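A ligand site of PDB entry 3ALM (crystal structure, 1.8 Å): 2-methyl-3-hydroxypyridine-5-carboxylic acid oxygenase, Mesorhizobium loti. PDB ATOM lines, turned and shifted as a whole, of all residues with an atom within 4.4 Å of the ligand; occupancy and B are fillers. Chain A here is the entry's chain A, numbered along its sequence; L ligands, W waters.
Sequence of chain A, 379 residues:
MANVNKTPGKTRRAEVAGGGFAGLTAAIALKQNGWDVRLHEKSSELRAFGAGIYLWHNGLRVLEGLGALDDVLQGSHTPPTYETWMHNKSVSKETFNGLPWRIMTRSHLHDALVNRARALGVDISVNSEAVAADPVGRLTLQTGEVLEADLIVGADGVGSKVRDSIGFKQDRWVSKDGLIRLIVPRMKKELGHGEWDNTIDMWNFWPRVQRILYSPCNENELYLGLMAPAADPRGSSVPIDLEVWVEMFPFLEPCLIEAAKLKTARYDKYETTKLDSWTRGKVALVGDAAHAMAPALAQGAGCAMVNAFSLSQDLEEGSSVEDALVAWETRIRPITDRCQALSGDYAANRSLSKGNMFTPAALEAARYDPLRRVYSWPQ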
ATOM      1  N   ALA A  17     -35.909 -28.433  14.732  1.00  0.00           N
ATOM      2  CA  ALA A  17     -35.199 -29.632  14.311  1.00  0.00           C
ATOM      3  C   ALA A  17     -34.058 -29.189  13.362  1.00  0.00           C
ATOM      4  O   ALA A  17     -34.354 -28.640  12.279  1.00  0.00           O
ATOM      5  CB  ALA A  17     -36.145 -30.531  13.527  1.00  0.00           C
ATOM      6  N   GLY A  18     -32.808 -29.434  13.751  1.00  0.00           N
ATOM      7  CA  GLY A  18     -31.631 -29.098  12.907  1.00  0.00           C
ATOM      8  C   GLY A  18     -30.793 -28.039  13.522  1.00  0.00           C
ATOM      9  O   GLY A  18     -31.294 -26.968  13.813  1.00  0.00           O
ATOM     10  N   GLY A  19     -29.510 -28.351  13.724  1.00  0.00           N
ATOM     11  CA  GLY A  19     -28.582 -27.320  14.205  1.00  0.00           C
ATOM     12  C   GLY A  19     -27.646 -26.824  13.129  1.00  0.00           C
ATOM     13  O   GLY A  19     -26.441 -26.671  13.343  1.00  0.00           O
ATOM     14  N   GLY A  20     -28.221 -26.506  11.946  1.00  0.00           N
ATOM     15  CA  GLY A  20     -27.368 -25.917  10.906  1.00  0.00           C
ATOM     16  C   GLY A  20     -27.558 -24.434  10.923  1.00  0.00           C
ATOM     17  O   GLY A  20     -28.101 -23.834  11.891  1.00  0.00           O
ATOM     18  N   PHE A  21     -27.092 -23.760   9.867  1.00  0.00           N
ATOM     19  CA  PHE A  21     -27.280 -22.276   9.945  1.00  0.00           C
ATOM     20  C   PHE A  21     -28.769 -21.813  10.074  1.00  0.00           C
ATOM     21  O   PHE A  21     -29.063 -20.818  10.766  1.00  0.00           O
ATOM     22  CB  PHE A  21     -26.643 -21.649   8.668  1.00  0.00           C
ATOM     23  CG  PHE A  21     -25.228 -22.013   8.510  1.00  0.00           C
ATOM     24  CD1 PHE A  21     -24.290 -21.846   9.579  1.00  0.00           C
ATOM     25  CD2 PHE A  21     -24.781 -22.620   7.346  1.00  0.00           C
ATOM     26  CE1 PHE A  21     -22.963 -22.145   9.410  1.00  0.00           C
ATOM     27  CE2 PHE A  21     -23.431 -22.956   7.190  1.00  0.00           C
ATOM     28  CZ  PHE A  21     -22.524 -22.734   8.236  1.00  0.00           C
ATOM     29  N   ALA A  22     -29.673 -22.514   9.397  1.00  0.00           N
ATOM     30  CA  ALA A  22     -31.130 -22.128   9.440  1.00  0.00           C
ATOM     31  C   ALA A  22     -31.708 -22.324  10.857  1.00  0.00           C
ATOM     32  O   ALA A  22     -32.358 -21.431  11.430  1.00  0.00           O
ATOM     33  CB  ALA A  22     -31.946 -22.896   8.402  1.00  0.00           C
ATOM     34  N   GLY A  23     -31.460 -23.495  11.433  1.00  0.00           N
ATOM     35  CA  GLY A  23     -31.927 -23.823  12.791  1.00  0.00           C
ATOM     36  C   GLY A  23     -31.330 -22.920  13.850  1.00  0.00           C
ATOM     37  O   GLY A  23     -32.069 -22.450  14.748  1.00  0.00           O
ATOM     38  N   HIS A  40     -32.836 -29.297  18.333  1.00  0.00           N
ATOM     39  CA  HIS A  40     -32.463 -30.728  18.295  1.00  0.00           C
ATOM     40  C   HIS A  40     -31.531 -30.953  17.094  1.00  0.00           C
ATOM     41  O   HIS A  40     -31.929 -30.708  15.926  1.00  0.00           O
ATOM     42  CB  HIS A  40     -33.740 -31.604  18.186  1.00  0.00           C
ATOM     43  CG  HIS A  40     -34.655 -31.427  19.337  1.00  0.00           C
ATOM     44  ND1 HIS A  40     -34.565 -32.195  20.493  1.00  0.00           N
ATOM     45  CD2 HIS A  40     -35.627 -30.517  19.569  1.00  0.00           C
ATOM     46  CE1 HIS A  40     -35.433 -31.756  21.379  1.00  0.00           C
ATOM     47  NE2 HIS A  40     -36.097 -30.735  20.841  1.00  0.00           N
ATOM     48  N   GLU A  41     -30.336 -31.440  17.354  1.00  0.00           N
ATOM     49  CA  GLU A  41     -29.368 -31.775  16.330  1.00  0.00           C
ATOM     50  C   GLU A  41     -29.135 -33.285  16.301  1.00  0.00           C
ATOM     51  O   GLU A  41     -28.721 -33.898  17.353  1.00  0.00           O
ATOM     52  CB  GLU A  41     -28.050 -30.983  16.603  1.00  0.00           C
ATOM     53  CG  GLU A  41     -26.843 -31.520  15.799  1.00  0.00           C
ATOM     54  CD  GLU A  41     -27.104 -31.533  14.270  1.00  0.00           C
ATOM     55  OE1 GLU A  41     -26.862 -32.541  13.584  1.00  0.00           O
ATOM     56  OE2 GLU A  41     -27.623 -30.518  13.795  1.00  0.00           O
ATOM     57  N   LYS A  42     -29.353 -33.920  15.140  1.00  0.00           N
ATOM     58  CA  LYS A  42     -29.240 -35.362  15.069  1.00  0.00           C
ATOM     59  C   LYS A  42     -27.827 -35.862  15.321  1.00  0.00           C
ATOM     60  O   LYS A  42     -27.647 -36.959  15.906  1.00  0.00           O
ATOM     61  CB  LYS A  42     -29.823 -35.972  13.765  1.00  0.00           C
ATOM     62  CG  LYS A  42     -28.910 -35.970  12.592  1.00  0.00           C
ATOM     63  CD  LYS A  42     -29.443 -36.858  11.439  1.00  0.00           C
ATOM     64  CE  LYS A  42     -28.404 -36.705  10.263  1.00  0.00           C
ATOM     65  NZ  LYS A  42     -28.829 -37.022   8.831  1.00  0.00           N
ATOM     66  N   ILE A  53     -17.473 -20.686   3.294  1.00  0.00           N
ATOM     67  CA  ILE A  53     -18.788 -20.089   2.930  1.00  0.00           C
ATOM     68  C   ILE A  53     -18.656 -18.613   2.647  1.00  0.00           C
ATOM     69  O   ILE A  53     -17.903 -17.897   3.241  1.00  0.00           O
ATOM     70  CB  ILE A  53     -19.877 -20.370   4.042  1.00  0.00           C
ATOM     71  CG1 ILE A  53     -21.300 -20.192   3.500  1.00  0.00           C
ATOM     72  CG2 ILE A  53     -19.582 -19.611   5.380  1.00  0.00           C
ATOM     73  CD1 ILE A  53     -22.431 -20.670   4.505  1.00  0.00           C
ATOM     74  N   TYR A  54     -19.469 -18.139   1.719  1.00  0.00           N
ATOM     75  CA  TYR A  54     -19.554 -16.729   1.509  1.00  0.00           C
ATOM     76  C   TYR A  54     -20.890 -16.167   2.096  1.00  0.00           C
ATOM     77  O   TYR A  54     -21.925 -16.815   1.978  1.00  0.00           O
ATOM     78  CB  TYR A  54     -19.727 -16.513  -0.040  1.00  0.00           C
ATOM     79  CG  TYR A  54     -18.447 -16.516  -0.857  1.00  0.00           C
ATOM     80  CD1 TYR A  54     -17.691 -17.671  -0.995  1.00  0.00           C
ATOM     81  CD2 TYR A  54     -18.043 -15.367  -1.614  1.00  0.00           C
ATOM     82  CE1 TYR A  54     -16.525 -17.692  -1.783  1.00  0.00           C
ATOM     83  CE2 TYR A  54     -16.873 -15.412  -2.438  1.00  0.00           C
ATOM     84  CZ  TYR A  54     -16.091 -16.570  -2.464  1.00  0.00           C
ATOM     85  OH  TYR A  54     -14.927 -16.710  -3.199  1.00  0.00           O
ATOM     86  N   LEU A  55     -20.839 -14.968   2.715  1.00  0.00           N
ATOM     87  CA  LEU A  55     -21.979 -14.277   3.172  1.00  0.00           C
ATOM     88  C   LEU A  55     -21.985 -12.887   2.474  1.00  0.00           C
ATOM     89  O   LEU A  55     -20.938 -12.347   2.146  1.00  0.00           O
ATOM     90  CB  LEU A  55     -22.028 -14.051   4.678  1.00  0.00           C
ATOM     91  CG  LEU A  55     -22.335 -15.355   5.463  1.00  0.00           C
ATOM     92  CD1 LEU A  55     -22.524 -14.894   6.931  1.00  0.00           C
ATOM     93  CD2 LEU A  55     -23.605 -16.139   4.967  1.00  0.00           C
ATOM     94  N   ARG A 106     -16.698 -22.487   7.287  1.00  0.00           N
ATOM     95  CA  ARG A 106     -17.947 -22.911   7.840  1.00  0.00           C
ATOM     96  C   ARG A 106     -17.882 -22.995   9.337  1.00  0.00           C
ATOM     97  O   ARG A 106     -18.811 -22.641  10.015  1.00  0.00           O
ATOM     98  CB  ARG A 106     -18.347 -24.296   7.246  1.00  0.00           C
ATOM     99  CG  ARG A 106     -18.651 -24.281   5.686  1.00  0.00           C
ATOM    100  CD  ARG A 106     -20.068 -24.311   5.386  1.00  0.00           C
ATOM    101  NE  ARG A 106     -20.351 -24.146   3.931  1.00  0.00           N
ATOM    102  CZ  ARG A 106     -21.555 -24.285   3.403  1.00  0.00           C
ATOM    103  NH1 ARG A 106     -22.579 -24.653   4.176  1.00  0.00           N
ATOM    104  NH2 ARG A 106     -21.726 -24.071   2.097  1.00  0.00           N
ATOM    105  N   SER A 128     -30.134 -35.999  18.763  1.00  0.00           N
ATOM    106  CA  SER A 128     -31.501 -35.838  19.020  1.00  0.00           C
ATOM    107  C   SER A 128     -32.144 -35.574  17.675  1.00  0.00           C
ATOM    108  O   SER A 128     -31.980 -34.467  17.122  1.00  0.00           O
ATOM    109  CB  SER A 128     -31.697 -34.659  19.990  1.00  0.00           C
ATOM    110  OG  SER A 128     -33.045 -34.465  20.363  1.00  0.00           O
ATOM    111  N   GLU A 129     -32.786 -36.614  17.156  1.00  0.00           N
ATOM    112  CA  GLU A 129     -33.246 -36.600  15.737  1.00  0.00           C
ATOM    113  C   GLU A 129     -34.744 -36.500  15.699  1.00  0.00           C
ATOM    114  O   GLU A 129     -35.464 -37.339  16.218  1.00  0.00           O
ATOM    115  CB  GLU A 129     -32.739 -37.868  15.034  1.00  0.00           C
ATOM    116  CG  GLU A 129     -33.284 -38.032  13.577  1.00  0.00           C
ATOM    117  CD  GLU A 129     -32.888 -39.344  12.881  1.00  0.00           C
ATOM    118  OE1 GLU A 129     -32.337 -40.281  13.522  1.00  0.00           O
ATOM    119  OE2 GLU A 129     -33.095 -39.443  11.672  1.00  0.00           O
ATOM    120  N   ALA A 130     -35.257 -35.502  14.960  1.00  0.00           N
ATOM    121  CA  ALA A 130     -36.643 -35.408  14.693  1.00  0.00           C
ATOM    122  C   ALA A 130     -36.985 -36.409  13.590  1.00  0.00           C
ATOM    123  O   ALA A 130     -36.318 -36.420  12.540  1.00  0.00           O
ATOM    124  CB  ALA A 130     -36.921 -34.020  14.149  1.00  0.00           C
ATOM    125  N   ALA A 155     -35.808 -27.260  10.168  1.00  0.00           N
ATOM    126  CA  ALA A 155     -34.503 -26.699   9.713  1.00  0.00           C
ATOM    127  C   ALA A 155     -33.542 -27.875   9.541  1.00  0.00           C
ATOM    128  O   ALA A 155     -32.317 -27.732   9.791  1.00  0.00           O
ATOM    129  CB  ALA A 155     -33.960 -25.635  10.770  1.00  0.00           C
ATOM    130  N   ASP A 156     -34.077 -29.035   9.099  1.00  0.00           N
ATOM    131  CA  ASP A 156     -33.277 -30.264   9.128  1.00  0.00           C
ATOM    132  C   ASP A 156     -32.626 -30.628   7.787  1.00  0.00           C
ATOM    133  O   ASP A 156     -32.100 -31.742   7.627  1.00  0.00           O
ATOM    134  CB  ASP A 156     -34.115 -31.431   9.791  1.00  0.00           C
ATOM    135  CG  ASP A 156     -35.480 -31.596   9.174  1.00  0.00           C
ATOM    136  OD1 ASP A 156     -36.083 -30.590   8.600  1.00  0.00           O
ATOM    137  OD2 ASP A 156     -35.986 -32.702   9.254  1.00  0.00           O
ATOM    138  N   GLY A 157     -32.629 -29.640   6.852  1.00  0.00           N
ATOM    139  CA  GLY A 157     -31.782 -29.755   5.639  1.00  0.00           C
ATOM    140  C   GLY A 157     -32.389 -30.583   4.505  1.00  0.00           C
ATOM    141  O   GLY A 157     -33.576 -30.968   4.519  1.00  0.00           O
ATOM    142  N   LYS A 161     -36.843 -35.093   7.213  1.00  0.00           N
ATOM    143  CA  LYS A 161     -37.945 -35.878   7.797  1.00  0.00           C
ATOM    144  C   LYS A 161     -39.122 -35.061   8.302  1.00  0.00           C
ATOM    145  O   LYS A 161     -40.284 -35.548   8.281  1.00  0.00           O
ATOM    146  CB  LYS A 161     -37.334 -36.774   8.922  1.00  0.00           C
ATOM    147  CG  LYS A 161     -36.450 -37.763   8.326  1.00  0.00           C
ATOM    148  CD  LYS A 161     -35.840 -38.664   9.465  1.00  0.00           C
ATOM    149  CE  LYS A 161     -35.330 -39.901   8.874  1.00  0.00           C
ATOM    150  NZ  LYS A 161     -34.661 -40.785   9.956  1.00  0.00           N
ATOM    151  N   LEU A 179     -18.187 -30.953  -6.573  1.00  0.00           N
ATOM    152  CA  LEU A 179     -16.867 -30.366  -6.376  1.00  0.00           C
ATOM    153  C   LEU A 179     -16.318 -30.812  -5.048  1.00  0.00           C
ATOM    154  O   LEU A 179     -17.004 -31.438  -4.219  1.00  0.00           O
ATOM    155  CB  LEU A 179     -16.931 -28.817  -6.380  1.00  0.00           C
ATOM    156  CG  LEU A 179     -17.495 -28.138  -5.072  1.00  0.00           C
ATOM    157  CD1 LEU A 179     -17.331 -26.624  -5.170  1.00  0.00           C
ATOM    158  CD2 LEU A 179     -19.018 -28.504  -4.844  1.00  0.00           C
ATOM    159  N   ARG A 181     -14.497 -29.387  -1.761  1.00  0.00           N
ATOM    160  CA  ARG A 181     -14.280 -28.175  -0.991  1.00  0.00           C
ATOM    161  C   ARG A 181     -13.350 -28.435   0.173  1.00  0.00           C
ATOM    162  O   ARG A 181     -13.665 -29.390   0.913  1.00  0.00           O
ATOM    163  CB  ARG A 181     -15.626 -27.724  -0.431  1.00  0.00           C
ATOM    164  CG  ARG A 181     -16.439 -27.050  -1.550  1.00  0.00           C
ATOM    165  CD  ARG A 181     -17.873 -26.739  -1.106  1.00  0.00           C
ATOM    166  NE  ARG A 181     -18.624 -27.972  -0.804  1.00  0.00           N
ATOM    167  CZ  ARG A 181     -19.753 -28.020  -0.099  1.00  0.00           C
ATOM    168  NH1 ARG A 181     -20.356 -26.907   0.269  1.00  0.00           N
ATOM    169  NH2 ARG A 181     -20.315 -29.205   0.189  1.00  0.00           N
ATOM    170  N   TYR A 270     -25.112 -31.557  -5.468  1.00  0.00           N
ATOM    171  CA  TYR A 270     -26.106 -30.841  -4.696  1.00  0.00           C
ATOM    172  C   TYR A 270     -27.488 -31.156  -5.284  1.00  0.00           C
ATOM    173  O   TYR A 270     -27.574 -31.680  -6.439  1.00  0.00           O
ATOM    174  CB  TYR A 270     -25.827 -29.319  -4.694  1.00  0.00           C
ATOM    175  CG  TYR A 270     -26.015 -28.652  -6.066  1.00  0.00           C
ATOM    176  CD1 TYR A 270     -27.257 -28.134  -6.461  1.00  0.00           C
ATOM    177  CD2 TYR A 270     -24.908 -28.528  -6.971  1.00  0.00           C
ATOM    178  CE1 TYR A 270     -27.436 -27.563  -7.728  1.00  0.00           C
ATOM    179  CE2 TYR A 270     -25.087 -27.900  -8.273  1.00  0.00           C
ATOM    180  CZ  TYR A 270     -26.321 -27.443  -8.597  1.00  0.00           C
ATOM    181  OH  TYR A 270     -26.536 -26.800  -9.793  1.00  0.00           O
ATOM    182  N   VAL A 286     -37.678 -24.226   7.173  1.00  0.00           N
ATOM    183  CA  VAL A 286     -36.634 -23.180   6.773  1.00  0.00           C
ATOM    184  C   VAL A 286     -35.329 -23.769   6.272  1.00  0.00           C
ATOM    185  O   VAL A 286     -34.943 -24.949   6.561  1.00  0.00           O
ATOM    186  CB  VAL A 286     -36.306 -22.231   7.911  1.00  0.00           C
ATOM    187  CG1 VAL A 286     -37.591 -21.656   8.462  1.00  0.00           C
ATOM    188  CG2 VAL A 286     -35.733 -22.967   9.051  1.00  0.00           C
ATOM    189  N   GLY A 287     -34.643 -23.017   5.444  1.00  0.00           N
ATOM    190  CA  GLY A 287     -33.389 -23.433   4.901  1.00  0.00           C
ATOM    191  C   GLY A 287     -33.510 -24.491   3.784  1.00  0.00           C
ATOM    192  O   GLY A 287     -34.523 -24.561   3.071  1.00  0.00           O
ATOM    193  N   ASP A 288     -32.505 -25.377   3.710  1.00  0.00           N
ATOM    194  CA  ASP A 288     -32.457 -26.349   2.626  1.00  0.00           C
ATOM    195  C   ASP A 288     -33.687 -27.249   2.595  1.00  0.00           C
ATOM    196  O   ASP A 288     -34.046 -27.750   1.491  1.00  0.00           O
ATOM    197  CB  ASP A 288     -31.206 -27.228   2.686  1.00  0.00           C
ATOM    198  CG  ASP A 288     -29.991 -26.585   2.003  1.00  0.00           C
ATOM    199  OD1 ASP A 288     -30.052 -25.432   1.504  1.00  0.00           O
ATOM    200  OD2 ASP A 288     -28.954 -27.234   1.965  1.00  0.00           O
ATOM    201  N   PRO A 295     -25.639 -23.511  -6.187  1.00  0.00           N
ATOM    202  CA  PRO A 295     -24.659 -22.635  -5.481  1.00  0.00           C
ATOM    203  C   PRO A 295     -24.183 -21.373  -6.191  1.00  0.00           C
ATOM    204  O   PRO A 295     -23.498 -20.570  -5.531  1.00  0.00           O
ATOM    205  CB  PRO A 295     -23.437 -23.546  -5.219  1.00  0.00           C
ATOM    206  CG  PRO A 295     -23.653 -24.732  -6.033  1.00  0.00           C
ATOM    207  CD  PRO A 295     -25.042 -24.752  -6.675  1.00  0.00           C
ATOM    208  N   ALA A 298     -24.208 -18.052  -4.370  1.00  0.00           N
ATOM    209  CA  ALA A 298     -23.689 -18.015  -3.013  1.00  0.00           C
ATOM    210  C   ALA A 298     -24.699 -17.391  -2.047  1.00  0.00           C
ATOM    211  O   ALA A 298     -24.366 -16.567  -1.190  1.00  0.00           O
ATOM    212  CB  ALA A 298     -22.279 -17.315  -2.893  1.00  0.00           C
ATOM    213  N   GLN A 299     -25.938 -17.892  -2.131  1.00  0.00           N
ATOM    214  CA  GLN A 299     -27.089 -17.362  -1.383  1.00  0.00           C
ATOM    215  C   GLN A 299     -27.910 -18.453  -0.696  1.00  0.00           C
ATOM    216  O   GLN A 299     -28.920 -18.158  -0.080  1.00  0.00           O
ATOM    217  CB  GLN A 299     -28.033 -16.527  -2.296  1.00  0.00           C
ATOM    218  CG  GLN A 299     -27.550 -15.135  -2.345  1.00  0.00           C
ATOM    219  CD  GLN A 299     -27.721 -14.362  -1.049  1.00  0.00           C
ATOM    220  OE1 GLN A 299     -28.587 -14.630  -0.270  1.00  0.00           O
ATOM    221  NE2 GLN A 299     -26.855 -13.286  -0.863  1.00  0.00           N
ATOM    222  N   GLY A 300     -27.476 -19.723  -0.748  1.00  0.00           N
ATOM    223  CA  GLY A 300     -28.287 -20.771  -0.099  1.00  0.00           C
ATOM    224  C   GLY A 300     -28.454 -20.459   1.407  1.00  0.00           C
ATOM    225  O   GLY A 300     -29.585 -20.465   1.991  1.00  0.00           O
ATOM    226  N   ALA A 301     -27.300 -20.329   2.099  1.00  0.00           N
ATOM    227  CA  ALA A 301     -27.406 -20.011   3.509  1.00  0.00           C
ATOM    228  C   ALA A 301     -27.874 -18.571   3.779  1.00  0.00           C
ATOM    229  O   ALA A 301     -28.554 -18.353   4.807  1.00  0.00           O
ATOM    230  CB  ALA A 301     -26.064 -20.333   4.312  1.00  0.00           C
ATOM    231  N   GLY A 302     -27.534 -17.632   2.880  1.00  0.00           N
ATOM    232  CA  GLY A 302     -27.973 -16.244   3.100  1.00  0.00           C
ATOM    233  C   GLY A 302     -29.493 -16.240   3.105  1.00  0.00           C
ATOM    234  O   GLY A 302     -30.126 -15.626   3.981  1.00  0.00           O
HETATM  235  P1  LIG L   1     -27.901 -27.821   6.846  1.00  0.00           P
HETATM  236  O1  LIG L   1     -26.744 -26.908   6.831  1.00  0.00           O
HETATM  237  O2  LIG L   1     -27.970 -29.052   5.971  1.00  0.00           O
HETATM  238  O3  LIG L   1     -28.097 -28.240   8.459  1.00  0.00           O
HETATM  239  C1  LIG L   1     -29.183 -29.058   8.849  1.00  0.00           C
HETATM  240  C2  LIG L   1     -28.676 -29.643  10.206  1.00  0.00           C
HETATM  241  O4  LIG L   1     -29.786 -30.497  10.561  1.00  0.00           O
HETATM  242  C3  LIG L   1     -27.386 -30.525  10.120  1.00  0.00           C
HETATM  243  O5  LIG L   1     -26.598 -30.196  11.277  1.00  0.00           O
HETATM  244  C4  LIG L   1     -27.953 -31.936  10.201  1.00  0.00           C
HETATM  245  O6  LIG L   1     -27.084 -32.841  10.946  1.00  0.00           O
HETATM  246  C5  LIG L   1     -29.215 -31.749  11.030  1.00  0.00           C
HETATM  247  N1  LIG L   1     -30.270 -32.740  10.801  1.00  0.00           N
HETATM  248  C6  LIG L   1     -30.514 -33.457   9.680  1.00  0.00           C
HETATM  249  N2  LIG L   1     -31.592 -34.255   9.862  1.00  0.00           N
HETATM  250  C7  LIG L   1     -32.001 -34.020  11.133  1.00  0.00           C
HETATM  251  C8  LIG L   1     -33.021 -34.505  11.909  1.00  0.00           C
HETATM  252  N3  LIG L   1     -33.861 -35.396  11.373  1.00  0.00           N
HETATM  253  N4  LIG L   1     -33.210 -34.078  13.167  1.00  0.00           N
HETATM  254  C9  LIG L   1     -32.429 -33.164  13.712  1.00  0.00           C
HETATM  255  N5  LIG L   1     -31.429 -32.662  13.013  1.00  0.00           N
HETATM  256  C10 LIG L   1     -31.205 -33.057  11.716  1.00  0.00           C
HETATM  257  N6  LIG L   1     -24.666 -20.707   0.893  1.00  0.00           N
HETATM  258  C11 LIG L   1     -24.174 -19.487   1.142  1.00  0.00           C
HETATM  259  O7  LIG L   1     -24.898 -18.677   1.720  1.00  0.00           O
HETATM  260  N7  LIG L   1     -22.858 -19.126   0.791  1.00  0.00           N
HETATM  261  C12 LIG L   1     -22.114 -20.025   0.143  1.00  0.00           C
HETATM  262  O8  LIG L   1     -20.948 -19.731  -0.152  1.00  0.00           O
HETATM  263  C13 LIG L   1     -22.615 -21.278  -0.168  1.00  0.00           C
HETATM  264  N8  LIG L   1     -21.813 -22.168  -0.816  1.00  0.00           N
HETATM  265  C14 LIG L   1     -22.335 -23.368  -1.254  1.00  0.00           C
HETATM  266  C15 LIG L   1     -21.538 -24.257  -2.035  1.00  0.00           C
HETATM  267  C16 LIG L   1     -22.033 -25.490  -2.413  1.00  0.00           C
HETATM  268  C17 LIG L   1     -21.171 -26.431  -3.293  1.00  0.00           C
HETATM  269  C18 LIG L   1     -23.360 -25.845  -2.032  1.00  0.00           C
HETATM  270  C19 LIG L   1     -24.024 -27.228  -2.351  1.00  0.00           C
HETATM  271  C20 LIG L   1     -24.104 -25.017  -1.205  1.00  0.00           C
HETATM  272  C21 LIG L   1     -23.586 -23.768  -0.805  1.00  0.00           C
HETATM  273  N9  LIG L   1     -24.380 -22.910  -0.003  1.00  0.00           N
HETATM  274  C22 LIG L   1     -23.874 -21.637   0.240  1.00  0.00           C
HETATM  275  C23 LIG L   1     -25.693 -23.323   0.569  1.00  0.00           C
HETATM  276  C24 LIG L   1     -25.577 -23.771   2.030  1.00  0.00           C
HETATM  277  O9  LIG L   1     -24.586 -24.798   2.157  1.00  0.00           O
HETATM  278  C25 LIG L   1     -26.912 -24.337   2.540  1.00  0.00           C
HETATM  279  O10 LIG L   1     -27.996 -23.591   1.937  1.00  0.00           O
HETATM  280  C26 LIG L   1     -27.014 -24.161   4.027  1.00  0.00           C
HETATM  281  O11 LIG L   1     -25.907 -24.776   4.752  1.00  0.00           O
HETATM  282  C27 LIG L   1     -28.267 -24.842   4.532  1.00  0.00           C
HETATM  283  O12 LIG L   1     -28.510 -24.536   5.920  1.00  0.00           O
HETATM  284  P2  LIG L   1     -29.569 -25.457   6.718  1.00  0.00           P
HETATM  285  O13 LIG L   1     -29.529 -24.937   8.083  1.00  0.00           O
HETATM  286  O14 LIG L   1     -30.872 -25.209   5.949  1.00  0.00           O
HETATM  287  O15 LIG L   1     -29.262 -26.970   6.465  1.00  0.00           O
HETATM  288  O   HOH W   1     -26.947 -23.462  -2.458  1.00  0.00           O
HETATM  289  O   HOH W   2     -33.248 -26.792   6.461  1.00  0.00           O
HETATM  290  O   HOH W   3     -25.439 -21.110  -2.489  1.00  0.00           O
HETATM  291  O   HOH W   4     -32.285 -34.092   6.699  1.00  0.00           O
HETATM  292  O   HOH W   5     -30.420 -25.925  10.467  1.00  0.00           O
HETATM  293  O   HOH W   6     -28.988 -29.471   3.540  1.00  0.00           O
HETATM  294  O   HOH W   7     -18.859 -21.146  -1.468  1.00  0.00           O
HETATM  295  O   HOH W   8     -29.200 -24.087  -1.043  1.00  0.00           O
HETATM  296  O   HOH W   9     -34.063 -35.149   8.439  1.00  0.00           O
HETATM  297  O   HOH W  10     -24.515 -28.163  10.762  1.00  0.00           O
HETATM  298  O   HOH W  11     -25.309 -27.490   1.422  1.00  0.00           O
HETATM  299  O   HOH W  12     -19.407 -24.322   0.688  1.00  0.00           O
HETATM  300  O   HOH W  13     -30.988 -22.401   0.675  1.00  0.00           O
HETATM  301  O   HOH W  14     -25.141 -16.048   1.489  1.00  0.00           O
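An oxygen (O6) of the ligand is in hydrogen-bond range of the side-chain carboxylate (OE1) of Glu 41, at 2.7 Å.
The backbone NH (N) of Ala 22 is in hydrogen-bond range of an oxygen (O13) of the ligand, 2.8 Å away.
O8 of the ligand lies within hydrogen-bond range of N of Tyr 54, at 2.9 Å.
The backbone carbonyl oxygen (O) of Tyr 54 sits at hydrogen-bond distance from a nitrogen (N7) of the ligand (2.8 Å).
The backbone NH (N) of Asp 288 lies within hydrogen-bond range of an oxygen (O14) of the ligand.
OD1 of Asp 288 is in hydrogen-bond range of O10 of the ligand.
The guanidinium group of Arg 106 is in hydrogen-bond range of an oxygen (O9) of the ligand (2.9 Å).
N of Ala 130 sits at hydrogen-bond distance from N4 of the ligand (3.1 Å).
O of Ala 130 lies within hydrogen-bond range of N3 of the ligand, 2.9 Å away.
N of Ala 301 sits at hydrogen-bond distance from N6 of the ligand.
The backbone NH (N) of Gly 302 lies within hydrogen-bond range of an oxygen (O7) of the ligand (3.1 Å).
The backbone NH (N) of Gly 300 lies within hydrogen-bond range of a nitrogen (N6) of the ligand.
A nitrogen (N5) of the ligand is in hydrogen-bond range of the backbone NH of Lys 42, 3.2 Å away.
The backbone NH (N) of Phe 21 sits at hydrogen-bond distance from an oxygen (O13) of the ligand, at 3.2 Å.
N of Ser 128 lies within hydrogen-bond range of O of Glu 41, at 2.9 Å.
The side-chain carboxylate of Glu 41 lies within hydrogen-bond range of the backbone NH of Gly 19, at 2.9 Å.
OD2 of Asp 156 lies within hydrogen-bond range of N of Lys 161 (3.3 Å).
The backbone NH (N) of Lys 42 lies within hydrogen-bond range of the backbone carbonyl oxygen (O) of Ser 128 (3.3 Å).
N of Gly 18 is in hydrogen-bond range of O of His 40 (2.7 Å).
The side-chain hydroxyl (OG) of Ser 128 is in hydrogen-bond range of a ring nitrogen (ND1) of His 40, 2.7 Å away.
OE2 of Glu 129 lies within salt-bridge range of NZ of Lys 161.
The backbone NH (N) of Ala 155 is in hydrogen-bond range of the backbone carbonyl oxygen (O) of Ala 17, at 2.9 Å.
The backbone carbonyl oxygen of Asp 156 lies close to a nitrogen (N2) of the ligand.
Residues that only touch the ligand: Gly 18, Gly 19, Gly 20, His 40, Ile 53, Ser 128, Glu 129, Ala 155, Gly 157, Leu 179, Arg 181, Tyr 270, Gly 287, Pro 295, Ala 298 and Gln 299.
Hydrophobic or aromatic side chains within 4 Å of the ligand: Phe 21, Ala 22, Ile 53, Tyr 54, Ala 130, Leu 179, Tyr 270, Pro 295, Ala 298 and Ala 301.
Of the 33 residues printed, 28 come within 4 Å of the ligand.
Water W6 lies within hydrogen-bond range of an oxygen (O2) of the ligand (2.7 Å) and the side-chain carboxylate (OD2) of Asp 288 (2.7 Å).
Water W9 lies within hydrogen-bond range of N3 of the ligand (3.0 Å), N of Lys 161 (3.0 Å) and OD2 of Asp 156 (3.2 Å).
Water W3 lies within hydrogen-bond range of the backbone NH (N) of Gly 300 (3.0 Å), the backbone NH (N) of Gln 299 (3.3 Å) and a nitrogen (N6) of the ligand (3.5 Å).
Water W4 bridges the backbone carbonyl oxygen of Asp 156 (2.5 Å) and a nitrogen (N2) of the ligand (3.2 Å).
Water W12 bridges the guanidinium group of Arg 106 and the guanidinium group of Arg 181.
Water W13 lies within hydrogen-bond range of the backbone carbonyl oxygen of Gly 300 (2.7 Å), the side-chain carboxylate of Asp 288 (3.3 Å) and an oxygen (O10) of the ligand (3.5 Å).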
